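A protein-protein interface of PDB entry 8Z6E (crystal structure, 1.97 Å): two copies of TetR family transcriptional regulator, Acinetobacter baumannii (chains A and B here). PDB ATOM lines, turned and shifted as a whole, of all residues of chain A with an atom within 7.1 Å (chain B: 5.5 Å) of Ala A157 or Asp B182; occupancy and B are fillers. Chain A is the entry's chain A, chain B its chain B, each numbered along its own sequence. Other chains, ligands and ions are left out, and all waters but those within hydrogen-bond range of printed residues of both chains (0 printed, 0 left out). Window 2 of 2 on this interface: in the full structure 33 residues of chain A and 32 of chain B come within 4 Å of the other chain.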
ATOM      1  N   TYR A 143      30.126  -2.936  12.774  1.00  0.00           N
ATOM      2  CA  TYR A 143      30.662  -1.643  12.358  1.00  0.00           C
ATOM      3  C   TYR A 143      31.965  -1.339  13.083  1.00  0.00           C
ATOM      4  O   TYR A 143      32.925  -0.843  12.481  1.00  0.00           O
ATOM      5  CB  TYR A 143      29.642  -0.519  12.598  1.00  0.00           C
ATOM      6  CG  TYR A 143      30.197   0.870  12.282  1.00  0.00           C
ATOM      7  CD1 TYR A 143      30.939   1.567  13.228  1.00  0.00           C
ATOM      8  CD2 TYR A 143      29.991   1.472  11.039  1.00  0.00           C
ATOM      9  CE1 TYR A 143      31.475   2.817  12.955  1.00  0.00           C
ATOM     10  CE2 TYR A 143      30.522   2.739  10.762  1.00  0.00           C
ATOM     11  CZ  TYR A 143      31.267   3.391  11.731  1.00  0.00           C
ATOM     12  OH  TYR A 143      31.798   4.636  11.518  1.00  0.00           O
ATOM     13  N   ILE A 154      40.113   5.455   6.368  1.00  0.00           N
ATOM     14  CA  ILE A 154      38.878   5.783   5.663  1.00  0.00           C
ATOM     15  C   ILE A 154      38.022   6.595   6.630  1.00  0.00           C
ATOM     16  O   ILE A 154      37.935   6.258   7.815  1.00  0.00           O
ATOM     17  CB  ILE A 154      38.160   4.493   5.210  1.00  0.00           C
ATOM     18  CG1 ILE A 154      38.699   4.028   3.860  1.00  0.00           C
ATOM     19  CG2 ILE A 154      36.660   4.704   5.071  1.00  0.00           C
ATOM     20  CD1 ILE A 154      38.128   2.702   3.415  1.00  0.00           C
ATOM     21  N   ASN A 155      37.406   7.676   6.150  1.00  0.00           N
ATOM     22  CA  ASN A 155      36.755   8.562   7.111  1.00  0.00           C
ATOM     23  C   ASN A 155      35.395   8.005   7.545  1.00  0.00           C
ATOM     24  O   ASN A 155      34.865   7.045   6.974  1.00  0.00           O
ATOM     25  CB  ASN A 155      36.624   9.996   6.560  1.00  0.00           C
ATOM     26  CG  ASN A 155      35.739  10.098   5.319  1.00  0.00           C
ATOM     27  OD1 ASN A 155      34.782   9.344   5.136  1.00  0.00           O
ATOM     28  ND2 ASN A 155      36.058  11.057   4.465  1.00  0.00           N
ATOM     29  N   ASN A 156      34.830   8.628   8.583  1.00  0.00           N
ATOM     30  CA  ASN A 156      33.594   8.120   9.169  1.00  0.00           C
ATOM     31  C   ASN A 156      32.470   8.057   8.143  1.00  0.00           C
ATOM     32  O   ASN A 156      31.692   7.098   8.124  1.00  0.00           O
ATOM     33  CB  ASN A 156      33.184   8.985  10.356  1.00  0.00           C
ATOM     34  CG  ASN A 156      33.979   8.671  11.611  1.00  0.00           C
ATOM     35  OD1 ASN A 156      34.739   7.703  11.654  1.00  0.00           O
ATOM     36  ND2 ASN A 156      33.791   9.476  12.643  1.00  0.00           N
ATOM     37  N   ALA A 157      32.377   9.059   7.274  1.00  0.00           N
ATOM     38  CA  ALA A 157      31.321   9.074   6.270  1.00  0.00           C
ATOM     39  C   ALA A 157      31.422   7.872   5.337  1.00  0.00           C
ATOM     40  O   ALA A 157      30.415   7.226   5.034  1.00  0.00           O
ATOM     41  CB  ALA A 157      31.374  10.383   5.476  1.00  0.00           C
ATOM     42  N   ARG A 158      32.626   7.552   4.871  1.00  0.00           N
ATOM     43  CA  ARG A 158      32.762   6.396   3.992  1.00  0.00           C
ATOM     44  C   ARG A 158      32.568   5.095   4.755  1.00  0.00           C
ATOM     45  O   ARG A 158      32.032   4.132   4.204  1.00  0.00           O
ATOM     46  CB  ARG A 158      34.130   6.394   3.301  1.00  0.00           C
ATOM     47  CG  ARG A 158      34.129   7.140   1.990  1.00  0.00           C
ATOM     48  CD  ARG A 158      35.470   7.008   1.274  1.00  0.00           C
ATOM     49  NE  ARG A 158      35.939   8.304   0.806  1.00  0.00           N
ATOM     50  CZ  ARG A 158      36.865   9.015   1.437  1.00  0.00           C
ATOM     51  NH1 ARG A 158      37.448   8.563   2.545  1.00  0.00           N
ATOM     52  NH2 ARG A 158      37.237  10.192   0.932  1.00  0.00           N
ATOM     53  N   LEU A 159      32.980   5.049   6.020  1.00  0.00           N
ATOM     54  CA  LEU A 159      32.741   3.862   6.836  1.00  0.00           C
ATOM     55  C   LEU A 159      31.248   3.565   6.948  1.00  0.00           C
ATOM     56  O   LEU A 159      30.798   2.463   6.620  1.00  0.00           O
ATOM     57  CB  LEU A 159      33.366   4.048   8.218  1.00  0.00           C
ATOM     58  CG  LEU A 159      34.885   3.927   8.249  1.00  0.00           C
ATOM     59  CD1 LEU A 159      35.420   4.254   9.639  1.00  0.00           C
ATOM     60  CD2 LEU A 159      35.288   2.531   7.835  1.00  0.00           C
ATOM     61  N   ARG A 160      30.458   4.551   7.379  1.00  0.00           N
ATOM     62  CA  ARG A 160      29.019   4.329   7.533  1.00  0.00           C
ATOM     63  C   ARG A 160      28.362   3.928   6.217  1.00  0.00           C
ATOM     64  O   ARG A 160      27.464   3.080   6.200  1.00  0.00           O
ATOM     65  CB  ARG A 160      28.360   5.574   8.105  1.00  0.00           C
ATOM     66  CG  ARG A 160      28.628   5.782   9.596  1.00  0.00           C
ATOM     67  CD  ARG A 160      27.826   6.979  10.151  1.00  0.00           C
ATOM     68  NE  ARG A 160      28.178   8.252   9.522  1.00  0.00           N
ATOM     69  CZ  ARG A 160      29.038   9.136  10.014  1.00  0.00           C
ATOM     70  NH1 ARG A 160      29.697   8.913  11.140  1.00  0.00           N
ATOM     71  NH2 ARG A 160      29.245  10.271   9.354  1.00  0.00           N
ATOM     72  N   ILE A 161      28.792   4.520   5.105  1.00  0.00           N
ATOM     73  CA  ILE A 161      28.192   4.203   3.812  1.00  0.00           C
ATOM     74  C   ILE A 161      28.538   2.779   3.393  1.00  0.00           C
ATOM     75  O   ILE A 161      27.668   2.024   2.945  1.00  0.00           O
ATOM     76  CB  ILE A 161      28.636   5.228   2.754  1.00  0.00           C
ATOM     77  CG1 ILE A 161      27.854   6.529   2.912  1.00  0.00           C
ATOM     78  CG2 ILE A 161      28.489   4.661   1.341  1.00  0.00           C
ATOM     79  CD1 ILE A 161      28.497   7.685   2.196  1.00  0.00           C
ATOM     80  N   ILE A 162      29.808   2.386   3.534  1.00  0.00           N
ATOM     81  CA  ILE A 162      30.221   1.042   3.126  1.00  0.00           C
ATOM     82  C   ILE A 162      29.509  -0.021   3.951  1.00  0.00           C
ATOM     83  O   ILE A 162      28.985  -1.010   3.414  1.00  0.00           O
ATOM     84  CB  ILE A 162      31.756   0.902   3.233  1.00  0.00           C
ATOM     85  CG1 ILE A 162      32.427   1.729   2.172  1.00  0.00           C
ATOM     86  CG2 ILE A 162      32.163  -0.550   3.023  1.00  0.00           C
ATOM     87  CD1 ILE A 162      33.960   1.872   2.395  1.00  0.00           C
ATOM     88  N   LEU B 177      23.779   4.568  10.986  1.00  0.00           N
ATOM     89  CA  LEU B 177      23.201   4.855   9.681  1.00  0.00           C
ATOM     90  C   LEU B 177      23.945   5.976   8.958  1.00  0.00           C
ATOM     91  O   LEU B 177      24.303   6.986   9.567  1.00  0.00           O
ATOM     92  CB  LEU B 177      21.736   5.240   9.829  1.00  0.00           C
ATOM     93  CG  LEU B 177      20.877   4.040  10.234  1.00  0.00           C
ATOM     94  CD1 LEU B 177      19.381   4.401  10.153  1.00  0.00           C
ATOM     95  CD2 LEU B 177      21.204   2.832   9.387  1.00  0.00           C
ATOM     96  N   PRO B 178      24.151   5.846   7.655  1.00  0.00           N
ATOM     97  CA  PRO B 178      24.692   6.972   6.891  1.00  0.00           C
ATOM     98  C   PRO B 178      23.744   8.160   6.965  1.00  0.00           C
ATOM     99  O   PRO B 178      22.522   7.998   6.976  1.00  0.00           O
ATOM    100  CB  PRO B 178      24.803   6.414   5.466  1.00  0.00           C
ATOM    101  CG  PRO B 178      23.846   5.292   5.412  1.00  0.00           C
ATOM    102  CD  PRO B 178      23.719   4.735   6.795  1.00  0.00           C
ATOM    103  N   THR B 179      24.318   9.356   7.087  1.00  0.00           N
ATOM    104  CA  THR B 179      23.560  10.591   7.173  1.00  0.00           C
ATOM    105  C   THR B 179      23.427  11.190   5.790  1.00  0.00           C
ATOM    106  O   THR B 179      24.102  10.790   4.839  1.00  0.00           O
ATOM    107  CB  THR B 179      24.247  11.626   8.057  1.00  0.00           C
ATOM    108  OG1 THR B 179      25.556  11.872   7.539  1.00  0.00           O
ATOM    109  CG2 THR B 179      24.376  11.099   9.466  1.00  0.00           C
ATOM    110  N   TRP B 180      22.563  12.194   5.695  1.00  0.00           N
ATOM    111  CA  TRP B 180      22.465  12.922   4.442  1.00  0.00           C
ATOM    112  C   TRP B 180      23.807  13.549   4.078  1.00  0.00           C
ATOM    113  O   TRP B 180      24.244  13.476   2.925  1.00  0.00           O
ATOM    114  CB  TRP B 180      21.387  13.994   4.525  1.00  0.00           C
ATOM    115  CG  TRP B 180      21.576  15.018   3.476  1.00  0.00           C
ATOM    116  CD1 TRP B 180      21.841  16.342   3.655  1.00  0.00           C
ATOM    117  CD2 TRP B 180      21.535  14.801   2.057  1.00  0.00           C
ATOM    118  NE1 TRP B 180      21.950  16.972   2.435  1.00  0.00           N
ATOM    119  CE2 TRP B 180      21.769  16.043   1.439  1.00  0.00           C
ATOM    120  CE3 TRP B 180      21.318  13.677   1.252  1.00  0.00           C
ATOM    121  CZ2 TRP B 180      21.805  16.194   0.047  1.00  0.00           C
ATOM    122  CZ3 TRP B 180      21.357  13.833  -0.134  1.00  0.00           C
ATOM    123  CH2 TRP B 180      21.589  15.081  -0.714  1.00  0.00           C
ATOM    124  N   GLU B 181      24.490  14.142   5.054  1.00  0.00           N
ATOM    125  CA  GLU B 181      25.788  14.740   4.756  1.00  0.00           C
ATOM    126  C   GLU B 181      26.776  13.709   4.221  1.00  0.00           C
ATOM    127  O   GLU B 181      27.579  14.023   3.328  1.00  0.00           O
ATOM    128  CB  GLU B 181      26.344  15.451   5.985  1.00  0.00           C
ATOM    129  CG  GLU B 181      25.398  16.501   6.527  1.00  0.00           C
ATOM    130  CD  GLU B 181      26.036  17.865   6.525  1.00  0.00           C
ATOM    131  OE1 GLU B 181      27.286  17.926   6.513  1.00  0.00           O
ATOM    132  OE2 GLU B 181      25.304  18.883   6.515  1.00  0.00           O
ATOM    133  N   ASP B 182      26.702  12.464   4.721  1.00  0.00           N
ATOM    134  CA  ASP B 182      27.541  11.393   4.197  1.00  0.00           C
ATOM    135  C   ASP B 182      27.277  11.163   2.719  1.00  0.00           C
ATOM    136  O   ASP B 182      28.212  11.019   1.921  1.00  0.00           O
ATOM    137  CB  ASP B 182      27.297  10.092   4.967  1.00  0.00           C
ATOM    138  CG  ASP B 182      27.712  10.187   6.411  1.00  0.00           C
ATOM    139  OD1 ASP B 182      28.509  11.087   6.724  1.00  0.00           O
ATOM    140  OD2 ASP B 182      27.241   9.368   7.232  1.00  0.00           O
ATOM    141  N   ILE B 183      25.999  11.105   2.346  1.00  0.00           N
ATOM    142  CA  ILE B 183      25.607  10.756   0.987  1.00  0.00           C
ATOM    143  C   ILE B 183      25.885  11.906   0.024  1.00  0.00           C
ATOM    144  O   ILE B 183      26.237  11.682  -1.140  1.00  0.00           O
ATOM    145  CB  ILE B 183      24.123  10.347   0.979  1.00  0.00           C
ATOM    146  CG1 ILE B 183      23.960   8.981   1.643  1.00  0.00           C
ATOM    147  CG2 ILE B 183      23.574  10.297  -0.442  1.00  0.00           C
ATOM    148  CD1 ILE B 183      24.531   7.864   0.803  1.00  0.00           C
ATOM    149  N   GLU B 184      25.726  13.153   0.485  1.00  0.00           N
ATOM    150  CA  GLU B 184      26.007  14.302  -0.373  1.00  0.00           C
ATOM    151  C   GLU B 184      27.483  14.371  -0.745  1.00  0.00           C
ATOM    152  O   GLU B 184      27.830  14.874  -1.824  1.00  0.00           O
ATOM    153  CB  GLU B 184      25.584  15.602   0.309  1.00  0.00           C
ATOM    154  CG  GLU B 184      25.617  16.808  -0.642  1.00  0.00           C
ATOM    155  CD  GLU B 184      25.409  18.147   0.054  1.00  0.00           C
ATOM    156  OE1 GLU B 184      25.442  18.205   1.304  1.00  0.00           O
ATOM    157  OE2 GLU B 184      25.203  19.155  -0.657  1.00  0.00           O
ATOM    158  N   SER B 185      28.353  13.866   0.134  1.00  0.00           N
ATOM    159  CA  SER B 185      29.787  13.787  -0.150  1.00  0.00           C
ATOM    160  C   SER B 185      30.091  12.752  -1.231  1.00  0.00           C
ATOM    161  O   SER B 185      30.848  13.028  -2.168  1.00  0.00           O
ATOM    162  CB  SER B 185      30.550  13.454   1.133  1.00  0.00           C
ATOM    163  OG  SER B 185      30.365  14.480   2.096  1.00  0.00           O
ATOM    164  N   LEU B 186      29.560  11.538  -1.087  1.00  0.00           N
ATOM    165  CA  LEU B 186      29.606  10.569  -2.176  1.00  0.00           C
ATOM    166  C   LEU B 186      29.232  11.188  -3.513  1.00  0.00           C
ATOM    167  O   LEU B 186      29.935  11.015  -4.514  1.00  0.00           O
ATOM    168  CB  LEU B 186      28.667   9.400  -1.882  1.00  0.00           C
ATOM    169  CG  LEU B 186      29.035   8.115  -2.620  1.00  0.00           C
ATOM    170  CD1 LEU B 186      30.539   8.075  -2.838  1.00  0.00           C
ATOM    171  CD2 LEU B 186      28.552   6.896  -1.867  1.00  0.00           C
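Printed residues of chain A that touch a printed residue of chain B: Ala A157, Arg A160 and Ile A161.
Hydrophobic or aromatic side chains of chain A that line the printed part of chain B: Ala A157 and Ile A161.
Hydrophobic or aromatic side chains of chain B that line the printed part of chain A: Pro B178 and Leu B186.
Among the printed residues, 6 pairs touch across the chains.
Among the printed residues, Asp or Glu carboxylates within 4 Å of a Lys or Arg side-chain nitrogen of the other chain: Arg A160 with Asp B182.
No position is printed for both chains.
Of the 6 pairs that touch across the chains among the printed residues, none has its exchanged pair printed and touching as well.
The guanidinium group (NE) of Arg A160 is in salt-bridge range of the side-chain carboxylate (OD2) of Asp B182 (2.7 Å).
The backbone NH (N) of Ala A157 sits close to the side-chain amide oxygen (OD1) of Asn A155 (3.2 Å).
OD2 of Asp B182 is in hydrogen-bond range of N of Thr B179, at 2.9 Å.
Among the printed residues, pairs that only touch across the chains: Ala A157 with Asp B182, Arg A160 with Leu B177, Ile A161 with Pro B178, Ile A161 with Asp B182 and Ile A161 with Leu B186.
Asp B182 touches just these residues of chain A: Ala A157 (3.2 Å), Arg A160 (2.7 Å) and Ile A161 (3.4 Å).
Of the printed residues of chain A, Leu B177 touches Arg A160.
Of the printed residues of chain B, Ile A161 touches Pro B178 (3.98 Å), Asp B182 (3.4 Å) and Leu B186 (3.9 Å).
Printed residues of chain A within 4 Å of Pro B178: Ile A161 (3.98 Å).
Arg A158 touches none of the printed residues of chain B.
The nearest residue of chain B that does not touch Ala A157 is Ser B185 (5.4 Å).
The nearest printed residue of chain A that does not touch Pro B178 is Arg A160 (4.1 Å).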
